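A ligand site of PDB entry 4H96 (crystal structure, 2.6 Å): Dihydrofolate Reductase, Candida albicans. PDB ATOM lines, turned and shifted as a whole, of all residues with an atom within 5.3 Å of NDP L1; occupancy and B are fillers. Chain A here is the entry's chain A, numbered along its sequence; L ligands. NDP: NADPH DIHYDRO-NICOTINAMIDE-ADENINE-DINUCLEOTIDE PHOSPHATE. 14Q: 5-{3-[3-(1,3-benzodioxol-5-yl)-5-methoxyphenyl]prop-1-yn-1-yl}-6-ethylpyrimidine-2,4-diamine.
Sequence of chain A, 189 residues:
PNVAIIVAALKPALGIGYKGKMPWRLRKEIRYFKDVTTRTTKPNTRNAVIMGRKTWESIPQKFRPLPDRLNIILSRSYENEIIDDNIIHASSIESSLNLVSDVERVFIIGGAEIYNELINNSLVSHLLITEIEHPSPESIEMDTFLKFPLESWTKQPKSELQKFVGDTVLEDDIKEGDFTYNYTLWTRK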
ATOM      1  N   ILE A   6     -13.337  -9.899  11.123  1.00  0.00           N
ATOM      2  CA  ILE A   6     -12.786 -11.075  11.790  1.00  0.00           C
ATOM      3  C   ILE A   6     -13.861 -11.775  12.637  1.00  0.00           C
ATOM      4  O   ILE A   6     -14.524 -11.141  13.470  1.00  0.00           O
ATOM      5  CB  ILE A   6     -11.512 -10.723  12.632  1.00  0.00           C
ATOM      6  CG1 ILE A   6     -10.917 -11.988  13.282  1.00  0.00           C
ATOM      7  CG2 ILE A   6     -11.802  -9.628  13.662  1.00  0.00           C
ATOM      8  CD1 ILE A   6      -9.471 -11.838  13.722  1.00  0.00           C
ATOM      9  N   VAL A   7     -14.035 -13.074  12.391  1.00  0.00           N
ATOM     10  CA  VAL A   7     -15.096 -13.856  13.039  1.00  0.00           C
ATOM     11  C   VAL A   7     -14.713 -15.328  13.186  1.00  0.00           C
ATOM     12  O   VAL A   7     -13.954 -15.869  12.373  1.00  0.00           O
ATOM     13  CB  VAL A   7     -16.457 -13.702  12.277  1.00  0.00           C
ATOM     14  CG1 VAL A   7     -16.416 -14.362  10.893  1.00  0.00           C
ATOM     15  CG2 VAL A   7     -17.622 -14.228  13.098  1.00  0.00           C
ATOM     16  N   ALA A   8     -15.223 -15.969  14.234  1.00  0.00           N
ATOM     17  CA  ALA A   8     -15.056 -17.400  14.440  1.00  0.00           C
ATOM     18  C   ALA A   8     -16.411 -18.103  14.344  1.00  0.00           C
ATOM     19  O   ALA A   8     -17.316 -17.836  15.140  1.00  0.00           O
ATOM     20  CB  ALA A   8     -14.404 -17.679  15.788  1.00  0.00           C
ATOM     21  N   ALA A   9     -16.549 -18.983  13.354  1.00  0.00           N
ATOM     22  CA  ALA A   9     -17.825 -19.638  13.069  1.00  0.00           C
ATOM     23  C   ALA A   9     -17.707 -21.158  12.964  1.00  0.00           C
ATOM     24  O   ALA A   9     -16.680 -21.685  12.523  1.00  0.00           O
ATOM     25  CB  ALA A   9     -18.436 -19.069  11.791  1.00  0.00           C
ATOM     26  N   ILE A  16     -22.374 -18.578  15.832  1.00  0.00           N
ATOM     27  CA  ILE A  16     -21.419 -17.746  16.564  1.00  0.00           C
ATOM     28  C   ILE A  16     -21.696 -17.636  18.074  1.00  0.00           C
ATOM     29  O   ILE A  16     -20.761 -17.508  18.865  1.00  0.00           O
ATOM     30  CB  ILE A  16     -21.284 -16.315  15.966  1.00  0.00           C
ATOM     31  CG1 ILE A  16     -22.666 -15.737  15.607  1.00  0.00           C
ATOM     32  CG2 ILE A  16     -20.363 -16.336  14.758  1.00  0.00           C
ATOM     33  CD1 ILE A  16     -22.681 -14.228  15.388  1.00  0.00           C
ATOM     34  N   GLY A  17     -22.969 -17.680  18.451  1.00  0.00           N
ATOM     35  CA  GLY A  17     -23.347 -17.513  19.852  1.00  0.00           C
ATOM     36  C   GLY A  17     -24.628 -18.211  20.280  1.00  0.00           C
ATOM     37  O   GLY A  17     -25.449 -18.593  19.444  1.00  0.00           O
ATOM     38  N   TYR A  18     -24.779 -18.373  21.590  1.00  0.00           N
ATOM     39  CA  TYR A  18     -25.989 -18.950  22.176  1.00  0.00           C
ATOM     40  C   TYR A  18     -26.382 -18.188  23.436  1.00  0.00           C
ATOM     41  O   TYR A  18     -25.561 -18.019  24.348  1.00  0.00           O
ATOM     42  CB  TYR A  18     -25.799 -20.445  22.473  1.00  0.00           C
ATOM     43  CG  TYR A  18     -27.013 -21.117  23.074  1.00  0.00           C
ATOM     44  CD1 TYR A  18     -28.148 -21.382  22.295  1.00  0.00           C
ATOM     45  CD2 TYR A  18     -27.041 -21.503  24.417  1.00  0.00           C
ATOM     46  CE1 TYR A  18     -29.269 -22.000  22.839  1.00  0.00           C
ATOM     47  CE2 TYR A  18     -28.149 -22.121  24.968  1.00  0.00           C
ATOM     48  CZ  TYR A  18     -29.263 -22.369  24.179  1.00  0.00           C
ATOM     49  OH  TYR A  18     -30.367 -22.985  24.721  1.00  0.00           O
ATOM     50  N   GLY A  20     -26.862 -15.053  23.847  1.00  0.00           N
ATOM     51  CA  GLY A  20     -26.173 -13.761  23.974  1.00  0.00           C
ATOM     52  C   GLY A  20     -24.661 -13.841  24.113  1.00  0.00           C
ATOM     53  O   GLY A  20     -23.984 -12.810  24.030  1.00  0.00           O
ATOM     54  N   LYS A  21     -24.137 -15.040  24.333  1.00  0.00           N
ATOM     55  CA  LYS A  21     -22.686 -15.230  24.523  1.00  0.00           C
ATOM     56  C   LYS A  21     -22.123 -16.402  23.716  1.00  0.00           C
ATOM     57  O   LYS A  21     -22.863 -17.259  23.233  1.00  0.00           O
ATOM     58  CB  LYS A  21     -22.359 -15.377  26.016  1.00  0.00           C
ATOM     59  CG  LYS A  21     -22.375 -14.066  26.780  1.00  0.00           C
ATOM     60  CD  LYS A  21     -22.100 -14.263  28.261  1.00  0.00           C
ATOM     61  CE  LYS A  21     -22.239 -12.955  29.019  1.00  0.00           C
ATOM     62  NZ  LYS A  21     -22.077 -13.146  30.490  1.00  0.00           N
ATOM     63  N   MET A  22     -20.785 -16.423  23.587  1.00  0.00           N
ATOM     64  CA  MET A  22     -20.078 -17.439  22.822  1.00  0.00           C
ATOM     65  C   MET A  22     -20.159 -18.815  23.491  1.00  0.00           C
ATOM     66  O   MET A  22     -19.953 -18.929  24.703  1.00  0.00           O
ATOM     67  CB  MET A  22     -18.608 -17.025  22.641  1.00  0.00           C
ATOM     68  CG  MET A  22     -17.884 -17.730  21.499  1.00  0.00           C
ATOM     69  SD  MET A  22     -16.204 -17.124  21.275  1.00  0.00           S
ATOM     70  CE  MET A  22     -16.520 -15.374  21.017  1.00  0.00           C
ATOM     71  N   TRP A  24     -18.168 -21.359  23.007  1.00  0.00           N
ATOM     72  CA  TRP A  24     -16.851 -21.988  23.042  1.00  0.00           C
ATOM     73  C   TRP A  24     -15.764 -21.048  23.532  1.00  0.00           C
ATOM     74  O   TRP A  24     -15.852 -19.831  23.339  1.00  0.00           O
ATOM     75  CB  TRP A  24     -16.474 -22.575  21.669  1.00  0.00           C
ATOM     76  CG  TRP A  24     -16.584 -21.601  20.519  1.00  0.00           C
ATOM     77  CD1 TRP A  24     -15.762 -20.543  20.253  1.00  0.00           C
ATOM     78  CD2 TRP A  24     -17.574 -21.627  19.480  1.00  0.00           C
ATOM     79  NE1 TRP A  24     -16.185 -19.890  19.117  1.00  0.00           N
ATOM     80  CE2 TRP A  24     -17.291 -20.535  18.614  1.00  0.00           C
ATOM     81  CE3 TRP A  24     -18.666 -22.448  19.190  1.00  0.00           C
ATOM     82  CZ2 TRP A  24     -18.067 -20.253  17.486  1.00  0.00           C
ATOM     83  CZ3 TRP A  24     -19.435 -22.173  18.065  1.00  0.00           C
ATOM     84  CH2 TRP A  24     -19.129 -21.078  17.233  1.00  0.00           C
ATOM     85  N   MET A  51     -17.139  -2.413  17.018  1.00  0.00           N
ATOM     86  CA  MET A  51     -18.026  -3.410  17.613  1.00  0.00           C
ATOM     87  C   MET A  51     -19.429  -2.865  17.859  1.00  0.00           C
ATOM     88  O   MET A  51     -19.654  -1.652  17.800  1.00  0.00           O
ATOM     89  CB  MET A  51     -17.419  -3.947  18.917  1.00  0.00           C
ATOM     90  CG  MET A  51     -17.413  -2.963  20.075  1.00  0.00           C
ATOM     91  SD  MET A  51     -16.261  -3.418  21.381  1.00  0.00           S
ATOM     92  CE  MET A  51     -14.711  -2.827  20.683  1.00  0.00           C
ATOM     93  N   GLY A  52     -20.372  -3.769  18.125  1.00  0.00           N
ATOM     94  CA  GLY A  52     -21.738  -3.396  18.472  1.00  0.00           C
ATOM     95  C   GLY A  52     -21.874  -3.008  19.930  1.00  0.00           C
ATOM     96  O   GLY A  52     -20.922  -3.129  20.710  1.00  0.00           O
ATOM     97  N   ARG A  53     -23.063  -2.525  20.295  1.00  0.00           N
ATOM     98  CA  ARG A  53     -23.348  -2.101  21.674  1.00  0.00           C
ATOM     99  C   ARG A  53     -23.461  -3.307  22.616  1.00  0.00           C
ATOM    100  O   ARG A  53     -23.018  -3.237  23.764  1.00  0.00           O
ATOM    101  CB  ARG A  53     -24.626  -1.253  21.707  1.00  0.00           C
ATOM    102  CG  ARG A  53     -24.897  -0.578  23.046  1.00  0.00           C
ATOM    103  CD  ARG A  53     -26.225   0.183  23.028  1.00  0.00           C
ATOM    104  NE  ARG A  53     -27.369  -0.674  22.729  1.00  0.00           N
ATOM    105  CZ  ARG A  53     -28.050  -1.375  23.624  1.00  0.00           C
ATOM    106  NH1 ARG A  53     -27.731  -1.339  24.907  1.00  0.00           N
ATOM    107  NH2 ARG A  53     -29.080  -2.128  23.229  1.00  0.00           N
ATOM    108  N   LYS A  54     -24.048  -4.387  22.124  1.00  0.00           N
ATOM    109  CA  LYS A  54     -24.243  -5.600  22.912  1.00  0.00           C
ATOM    110  C   LYS A  54     -22.940  -6.381  23.140  1.00  0.00           C
ATOM    111  O   LYS A  54     -22.795  -7.055  24.168  1.00  0.00           O
ATOM    112  CB  LYS A  54     -25.297  -6.513  22.263  1.00  0.00           C
ATOM    113  CG  LYS A  54     -26.719  -5.972  22.352  1.00  0.00           C
ATOM    114  CD  LYS A  54     -27.701  -6.932  21.696  1.00  0.00           C
ATOM    115  CE  LYS A  54     -29.125  -6.383  21.774  1.00  0.00           C
ATOM    116  NZ  LYS A  54     -30.107  -7.310  21.136  1.00  0.00           N
ATOM    117  N   THR A  55     -22.022  -6.279  22.190  1.00  0.00           N
ATOM    118  CA  THR A  55     -20.704  -6.913  22.305  1.00  0.00           C
ATOM    119  C   THR A  55     -19.852  -6.198  23.350  1.00  0.00           C
ATOM    120  O   THR A  55     -19.159  -6.838  24.147  1.00  0.00           O
ATOM    121  CB  THR A  55     -19.969  -6.966  20.942  1.00  0.00           C
ATOM    122  OG1 THR A  55     -20.824  -7.570  19.960  1.00  0.00           O
ATOM    123  CG2 THR A  55     -18.684  -7.785  21.042  1.00  0.00           C
ATOM    124  N   LEU A  74     -20.733   1.037  17.915  1.00  0.00           N
ATOM    125  CA  LEU A  74     -21.826   1.494  17.068  1.00  0.00           C
ATOM    126  C   LEU A  74     -23.145   1.558  17.837  1.00  0.00           C
ATOM    127  O   LEU A  74     -23.583   0.563  18.417  1.00  0.00           O
ATOM    128  CB  LEU A  74     -21.980   0.612  15.820  1.00  0.00           C
ATOM    129  CG  LEU A  74     -20.942   0.722  14.705  1.00  0.00           C
ATOM    130  CD1 LEU A  74     -21.166  -0.369  13.680  1.00  0.00           C
ATOM    131  CD2 LEU A  74     -20.972   2.095  14.037  1.00  0.00           C
ATOM    132  N   SER A  75     -23.762   2.734  17.837  1.00  0.00           N
ATOM    133  CA  SER A  75     -25.061   2.947  18.483  1.00  0.00           C
ATOM    134  C   SER A  75     -25.834   4.068  17.798  1.00  0.00           C
ATOM    135  O   SER A  75     -25.264   5.118  17.485  1.00  0.00           O
ATOM    136  CB  SER A  75     -24.872   3.268  19.978  1.00  0.00           C
ATOM    137  OG  SER A  75     -26.120   3.337  20.636  1.00  0.00           O
ATOM    138  N   ARG A  76     -27.120   3.833  17.571  1.00  0.00           N
ATOM    139  CA  ARG A  76     -27.988   4.828  16.940  1.00  0.00           C
ATOM    140  C   ARG A  76     -28.456   5.893  17.945  1.00  0.00           C
ATOM    141  O   ARG A  76     -28.917   6.964  17.552  1.00  0.00           O
ATOM    142  CB  ARG A  76     -29.186   4.160  16.251  1.00  0.00           C
ATOM    143  CG  ARG A  76     -30.186   3.479  17.172  1.00  0.00           C
ATOM    144  CD  ARG A  76     -31.211   2.657  16.407  1.00  0.00           C
ATOM    145  NE  ARG A  76     -30.693   1.339  16.016  1.00  0.00           N
ATOM    146  CZ  ARG A  76     -30.231   1.038  14.802  1.00  0.00           C
ATOM    147  NH1 ARG A  76     -30.216   1.944  13.838  1.00  0.00           N
ATOM    148  NH2 ARG A  76     -29.795  -0.190  14.556  1.00  0.00           N
ATOM    149  N   SER A  77     -28.344   5.578  19.234  1.00  0.00           N
ATOM    150  CA  SER A  77     -28.727   6.490  20.310  1.00  0.00           C
ATOM    151  C   SER A  77     -27.663   7.562  20.552  1.00  0.00           C
ATOM    152  O   SER A  77     -27.986   8.724  20.786  1.00  0.00           O
ATOM    153  CB  SER A  77     -29.005   5.712  21.596  1.00  0.00           C
ATOM    154  OG  SER A  77     -30.019   4.741  21.409  1.00  0.00           O
ATOM    155  N   ALA A  90     -20.028   6.169  17.681  1.00  0.00           N
ATOM    156  CA  ALA A  90     -20.441   6.597  16.342  1.00  0.00           C
ATOM    157  C   ALA A  90     -21.746   5.928  15.905  1.00  0.00           C
ATOM    158  O   ALA A  90     -22.070   4.836  16.355  1.00  0.00           O
ATOM    159  CB  ALA A  90     -19.336   6.328  15.329  1.00  0.00           C
ATOM    160  N   SER A  91     -22.478   6.604  15.015  1.00  0.00           N
ATOM    161  CA  SER A  91     -23.746   6.099  14.500  1.00  0.00           C
ATOM    162  C   SER A  91     -23.542   5.090  13.363  1.00  0.00           C
ATOM    163  O   SER A  91     -24.231   4.075  13.295  1.00  0.00           O
ATOM    164  CB  SER A  91     -24.645   7.247  14.028  1.00  0.00           C
ATOM    165  OG  SER A  91     -24.024   7.991  12.986  1.00  0.00           O
ATOM    166  N   ILE A 109     -15.305  -6.717  14.906  1.00  0.00           N
ATOM    167  CA  ILE A 109     -15.177  -7.801  15.899  1.00  0.00           C
ATOM    168  C   ILE A 109     -16.498  -8.259  16.530  1.00  0.00           C
ATOM    169  O   ILE A 109     -16.497  -9.009  17.507  1.00  0.00           O
ATOM    170  CB  ILE A 109     -14.132  -7.446  16.999  1.00  0.00           C
ATOM    171  CG1 ILE A 109     -14.626  -6.276  17.874  1.00  0.00           C
ATOM    172  CG2 ILE A 109     -12.772  -7.131  16.374  1.00  0.00           C
ATOM    173  CD1 ILE A 109     -13.989  -6.229  19.250  1.00  0.00           C
ATOM    174  N   GLY A 110     -17.623  -7.807  15.971  1.00  0.00           N
ATOM    175  CA  GLY A 110     -18.947  -8.227  16.449  1.00  0.00           C
ATOM    176  C   GLY A 110     -19.977  -7.113  16.482  1.00  0.00           C
ATOM    177  O   GLY A 110     -19.633  -5.938  16.418  1.00  0.00           O
ATOM    178  N   GLY A 111     -21.249  -7.475  16.601  1.00  0.00           N
ATOM    179  CA  GLY A 111     -21.686  -8.873  16.660  1.00  0.00           C
ATOM    180  C   GLY A 111     -22.571  -9.254  15.487  1.00  0.00           C
ATOM    181  O   GLY A 111     -22.356  -8.790  14.364  1.00  0.00           O
ATOM    182  N   ALA A 112     -23.564 -10.095  15.751  1.00  0.00           N
ATOM    183  CA  ALA A 112     -24.458 -10.650  14.724  1.00  0.00           C
ATOM    184  C   ALA A 112     -25.166  -9.599  13.867  1.00  0.00           C
ATOM    185  O   ALA A 112     -25.253  -9.738  12.646  1.00  0.00           O
ATOM    186  CB  ALA A 112     -25.471 -11.585  15.357  1.00  0.00           C
ATOM    187  N   GLU A 113     -25.668  -8.552  14.523  1.00  0.00           N
ATOM    188  CA  GLU A 113     -26.370  -7.463  13.834  1.00  0.00           C
ATOM    189  C   GLU A 113     -25.394  -6.613  13.009  1.00  0.00           C
ATOM    190  O   GLU A 113     -25.772  -6.054  11.981  1.00  0.00           O
ATOM    191  CB  GLU A 113     -27.120  -6.586  14.835  1.00  0.00           C
ATOM    192  CG  GLU A 113     -28.240  -5.745  14.222  1.00  0.00           C
ATOM    193  CD  GLU A 113     -29.074  -5.014  15.269  1.00  0.00           C
ATOM    194  OE1 GLU A 113     -29.294  -5.574  16.361  1.00  0.00           O
ATOM    195  OE2 GLU A 113     -29.522  -3.888  14.983  1.00  0.00           O
ATOM    196  N   ILE A 114     -24.150  -6.544  13.469  1.00  0.00           N
ATOM    197  CA  ILE A 114     -23.090  -5.804  12.769  1.00  0.00           C
ATOM    198  C   ILE A 114     -22.541  -6.609  11.590  1.00  0.00           C
ATOM    199  O   ILE A 114     -22.335  -6.073  10.509  1.00  0.00           O
ATOM    200  CB  ILE A 114     -21.939  -5.404  13.739  1.00  0.00           C
ATOM    201  CG1 ILE A 114     -22.484  -4.721  15.011  1.00  0.00           C
ATOM    202  CG2 ILE A 114     -20.899  -4.520  13.030  1.00  0.00           C
ATOM    203  CD1 ILE A 114     -23.202  -3.392  14.796  1.00  0.00           C
ATOM    204  N   TYR A 115     -22.321  -7.919  11.810  1.00  0.00           N
ATOM    205  CA  TYR A 115     -21.783  -8.814  10.790  1.00  0.00           C
ATOM    206  C   TYR A 115     -22.663  -8.895   9.537  1.00  0.00           C
ATOM    207  O   TYR A 115     -22.164  -8.794   8.412  1.00  0.00           O
ATOM    208  CB  TYR A 115     -21.558 -10.220  11.346  1.00  0.00           C
ATOM    209  CG  TYR A 115     -20.375 -10.379  12.279  1.00  0.00           C
ATOM    210  CD1 TYR A 115     -19.127  -9.830  11.966  1.00  0.00           C
ATOM    211  CD2 TYR A 115     -20.484 -11.100  13.466  1.00  0.00           C
ATOM    212  CE1 TYR A 115     -18.038  -9.986  12.819  1.00  0.00           C
ATOM    213  CE2 TYR A 115     -19.405 -11.265  14.323  1.00  0.00           C
ATOM    214  CZ  TYR A 115     -18.178 -10.699  13.992  1.00  0.00           C
ATOM    215  OH  TYR A 115     -17.108 -10.862  14.834  1.00  0.00           O
ATOM    216  N   GLU A 117     -24.937  -6.853   8.380  1.00  0.00           N
ATOM    217  CA  GLU A 117     -25.146  -5.582   7.684  1.00  0.00           C
ATOM    218  C   GLU A 117     -23.880  -5.084   6.976  1.00  0.00           C
ATOM    219  O   GLU A 117     -23.966  -4.546   5.863  1.00  0.00           O
ATOM    220  CB  GLU A 117     -25.660  -4.514   8.655  1.00  0.00           C
ATOM    221  CG  GLU A 117     -27.095  -4.730   9.137  1.00  0.00           C
ATOM    222  CD  GLU A 117     -27.559  -3.683  10.117  1.00  0.00           C
ATOM    223  OE1 GLU A 117     -27.307  -2.471   9.889  1.00  0.00           O
ATOM    224  OE2 GLU A 117     -28.196  -4.050  11.127  1.00  0.00           O
ATOM    225  N   THR A 144     -27.997 -18.190  17.232  1.00  0.00           N
ATOM    226  CA  THR A 144     -27.428 -17.071  16.478  1.00  0.00           C
ATOM    227  C   THR A 144     -26.575 -17.605  15.328  1.00  0.00           C
ATOM    228  O   THR A 144     -25.632 -18.374  15.537  1.00  0.00           O
ATOM    229  CB  THR A 144     -26.580 -16.148  17.388  1.00  0.00           C
ATOM    230  OG1 THR A 144     -27.299 -15.862  18.595  1.00  0.00           O
ATOM    231  CG2 THR A 144     -26.274 -14.843  16.672  1.00  0.00           C
HETATM  232  PA  NDP L   1     -24.288  -6.672  18.363  1.00  0.00           P
HETATM  233  O1A NDP L   1     -24.403  -6.860  16.905  1.00  0.00           O
HETATM  234  O2A NDP L   1     -22.878  -6.642  18.785  1.00  0.00           O
HETATM  235  O5B NDP L   1     -25.028  -5.306  18.810  1.00  0.00           O
HETATM  236  C5B NDP L   1     -26.367  -5.044  18.462  1.00  0.00           C
HETATM  237  C4B NDP L   1     -26.717  -3.662  18.981  1.00  0.00           C
HETATM  238  O4B NDP L   1     -25.872  -2.693  18.373  1.00  0.00           O
HETATM  239  C3B NDP L   1     -28.152  -3.273  18.665  1.00  0.00           C
HETATM  240  O3B NDP L   1     -28.978  -3.492  19.787  1.00  0.00           O
HETATM  241  C2B NDP L   1     -28.057  -1.796  18.314  1.00  0.00           C
HETATM  242  O2B NDP L   1     -28.310  -1.019  19.466  1.00  0.00           O
HETATM  243  C1B NDP L   1     -26.614  -1.586  17.881  1.00  0.00           C
HETATM  244  N9A NDP L   1     -26.523  -1.537  16.409  1.00  0.00           N
HETATM  245  C8A NDP L   1     -26.596  -2.598  15.543  1.00  0.00           C
HETATM  246  N7A NDP L   1     -26.460  -2.149  14.276  1.00  0.00           N
HETATM  247  C5A NDP L   1     -26.309  -0.818  14.313  1.00  0.00           C
HETATM  248  C6A NDP L   1     -26.134   0.136  13.301  1.00  0.00           C
HETATM  249  N6A NDP L   1     -26.098  -0.235  12.033  1.00  0.00           N
HETATM  250  N1A NDP L   1     -25.995   1.470  13.637  1.00  0.00           N
HETATM  251  C2A NDP L   1     -26.033   1.859  14.974  1.00  0.00           C
HETATM  252  N3A NDP L   1     -26.212   0.908  15.963  1.00  0.00           N
HETATM  253  C4A NDP L   1     -26.343  -0.414  15.644  1.00  0.00           C
HETATM  254  O3  NDP L   1     -25.101  -7.826  19.147  1.00  0.00           O
HETATM  255  PN  NDP L   1     -25.818  -9.170  18.624  1.00  0.00           P
HETATM  256  O1N NDP L   1     -26.606  -9.740  19.749  1.00  0.00           O
HETATM  257  O2N NDP L   1     -26.485  -8.874  17.339  1.00  0.00           O
HETATM  258  O5D NDP L   1     -24.567 -10.142  18.329  1.00  0.00           O
HETATM  259  C5D NDP L   1     -23.719 -10.602  19.371  1.00  0.00           C
HETATM  260  C4D NDP L   1     -23.608 -12.119  19.297  1.00  0.00           C
HETATM  261  O4D NDP L   1     -22.591 -12.494  18.392  1.00  0.00           O
HETATM  262  C3D NDP L   1     -23.259 -12.710  20.656  1.00  0.00           C
HETATM  263  O3D NDP L   1     -24.243 -13.652  21.019  1.00  0.00           O
HETATM  264  C2D NDP L   1     -21.909 -13.368  20.477  1.00  0.00           C
HETATM  265  O2D NDP L   1     -21.893 -14.682  21.001  1.00  0.00           O
HETATM  266  C1D NDP L   1     -21.665 -13.394  18.977  1.00  0.00           C
HETATM  267  N1N NDP L   1     -20.274 -13.024  18.647  1.00  0.00           N
HETATM  268  C2N NDP L   1     -19.403 -13.999  18.243  1.00  0.00           C
HETATM  269  C3N NDP L   1     -18.083 -13.690  17.924  1.00  0.00           C
HETATM  270  C7N NDP L   1     -17.210 -14.708  17.253  1.00  0.00           C
HETATM  271  O7N NDP L   1     -16.319 -14.303  16.241  1.00  0.00           O
HETATM  272  N7N NDP L   1     -17.282 -15.989  17.638  1.00  0.00           N
HETATM  273  C4N NDP L   1     -17.662 -12.363  18.004  1.00  0.00           C
HETATM  274  C5N NDP L   1     -18.546 -11.374  18.404  1.00  0.00           C
HETATM  275  C6N NDP L   1     -19.858 -11.718  18.721  1.00  0.00           C
HETATM  276  P2B NDP L   1     -28.922   0.470  19.388  1.00  0.00           P
HETATM  277  O1X NDP L   1     -28.932   1.037  20.782  1.00  0.00           O
HETATM  278  O2X NDP L   1     -28.056   1.341  18.501  1.00  0.00           O
HETATM  279  O3X NDP L   1     -30.326   0.424  18.841  1.00  0.00           O
HETATM  280  CAY 14Q L   2     -11.672 -13.647  20.845  1.00  0.00           C
HETATM  281  CAH 14Q L   2     -12.946 -14.228  20.224  1.00  0.00           C
HETATM  282  C4  14Q L   2     -13.126 -13.727  18.786  1.00  0.00           C
HETATM  283  N3  14Q L   2     -12.485 -14.456  17.779  1.00  0.00           N
HETATM  284  C2  14Q L   2     -12.593 -14.088  16.423  1.00  0.00           C
HETATM  285  NAG 14Q L   2     -11.984 -14.786  15.484  1.00  0.00           N
HETATM  286  N1  14Q L   2     -13.354 -12.956  16.084  1.00  0.00           N
HETATM  287  C6  14Q L   2     -13.995 -12.227  17.091  1.00  0.00           C
HETATM  288  NAI 14Q L   2     -14.712 -11.151  16.753  1.00  0.00           N
HETATM  289  C5  14Q L   2     -13.878 -12.607  18.428  1.00  0.00           C
HETATM  290  CAJ 14Q L   2     -14.544 -11.829  19.442  1.00  0.00           C
HETATM  291  CAK 14Q L   2     -15.116 -11.175  20.301  1.00  0.00           C
HETATM  292  CAL 14Q L   2     -15.822 -10.354  21.303  1.00  0.00           C
HETATM  293  CAM 14Q L   2     -15.578 -10.872  22.723  1.00  0.00           C
HETATM  294  CAR 14Q L   2     -14.283 -11.055  23.199  1.00  0.00           C
HETATM  295  CAN 14Q L   2     -16.670 -11.152  23.545  1.00  0.00           C
HETATM  296  CAO 14Q L   2     -16.471 -11.617  24.851  1.00  0.00           C
HETATM  297  OAZ 14Q L   2     -17.536 -11.894  25.652  1.00  0.00           O
HETATM  298  CBA 14Q L   2     -17.984 -13.252  25.543  1.00  0.00           C
HETATM  299  CAP 14Q L   2     -15.165 -11.792  25.322  1.00  0.00           C
HETATM  300  CAQ 14Q L   2     -14.073 -11.526  24.498  1.00  0.00           C
HETATM  301  CAS 14Q L   2     -12.777 -11.709  24.974  1.00  0.00           C
HETATM  302  CAX 14Q L   2     -11.967 -10.609  25.253  1.00  0.00           C
HETATM  303  CAW 14Q L   2     -10.671 -10.792  25.729  1.00  0.00           C
HETATM  304  OBB 14Q L   2      -9.687  -9.903  26.068  1.00  0.00           O
HETATM  305  CBC 14Q L   2      -8.485 -10.668  25.989  1.00  0.00           C
HETATM  306  OBD 14Q L   2      -8.899 -11.982  26.378  1.00  0.00           O
HETATM  307  CAV 14Q L   2     -10.176 -12.081  25.919  1.00  0.00           C
HETATM  308  CAU 14Q L   2     -10.980 -13.188  25.643  1.00  0.00           C
HETATM  309  CAT 14Q L   2     -12.282 -12.998  25.165  1.00  0.00           C
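The backbone carbonyl oxygen (O) of Gly 20 sits close to an oxygen (O3D) of NDP L1 (3.1 Å). N of Gly 111 is in hydrogen-bond range of O2A of NDP L1, at 2.8 Å. The backbone NH (N) of Ala 8 is in hydrogen-bond range of an oxygen (O7N) of NDP L1 (2.8 Å). The backbone NH of Met 22 is in hydrogen-bond range of an oxygen (O2D) of NDP L1, at 3.3 Å. OH of Tyr 115 sits at hydrogen-bond distance from NAI of 14Q L2. The backbone NH (N) of Glu 113 lies within hydrogen-bond range of an oxygen (O2N) of NDP L1 (2.9 Å). NE of Arg 76 lies within salt-bridge range of O3X of NDP L1 (3.0 Å). The side-chain carboxylate (OE1) of Glu 117 is in hydrogen-bond range of a nitrogen (N6A) of NDP L1 (3.3 Å). NAI of 14Q L2 is in hydrogen-bond range of O of Ile 109 (2.9 Å). An oxygen (O5D) of NDP L1 lies within hydrogen-bond range of the backbone NH (N) of Ala 112. N of Arg 53 is in hydrogen-bond range of O4B of NDP L1 (3.4 Å). The backbone NH of Ile 114 lies close to an oxygen (O1A) of NDP L1. An oxygen (O2A) of NDP L1 sits at hydrogen-bond distance from the side-chain hydroxyl (OG1) of Thr 55. The guanidinium group (NE) of Arg 53 is in salt-bridge range of an oxygen (O1X) of NDP L1 (3.0 Å). O of Ile 6 sits at hydrogen-bond distance from NAI of 14Q L2 (3.3 Å). The backbone NH (N) of Arg 76 is in hydrogen-bond range of an oxygen (O2X) of NDP L1, at 2.8 Å. N7N of NDP L1 sits at hydrogen-bond distance from O of Ala 8.
OH of Tyr 115 sits close to O of Ile 109, at 3.3 Å. NE1 of Trp 24 sits at hydrogen-bond distance from SD of Met 22, at 3.5 Å. The backbone NH (N) of Ser 75 sits at hydrogen-bond distance from the backbone carbonyl oxygen (O) of Ala 90 (3.1 Å). The guanidinium group (NH2) of Arg 76 is in salt-bridge range of the side-chain carboxylate (OE2) of Glu 113, at 3.7 Å. The backbone NH of Leu 74 is in hydrogen-bond range of the backbone carbonyl oxygen of Met 51 (2.9 Å). The backbone NH (N) of Thr 144 sits close to the backbone carbonyl oxygen (O) of Gly 17, at 3.4 Å. OG1 of Thr 55 sits at hydrogen-bond distance from N of Gly 111 (3.4 Å). N of Ile 16 lies within hydrogen-bond range of O of Thr 144 (3.3 Å).
O of Ser 91 lies close to N1A of NDP L1. Residues that only touch NDP L1: Lys 21, Ile 109, Gly 17, Lys 54, Ser 75, Val 7, Gly 52, Ile 16, Tyr 115, Leu 74, Gly 110 and Ser 77. 24 residues have an atom within 4 Å of NDP L1: Val 7, Ala 8, Ile 16, Gly 17, Gly 20, Lys 21, Met 22, Gly 52, Arg 53, Lys 54, Thr 55, Leu 74, Ser 75, Arg 76, Ser 77, Ser 91, Ile 109, Gly 110, Gly 111, Ala 112, Glu 113, Ile 114, Tyr 115 and Glu 117.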
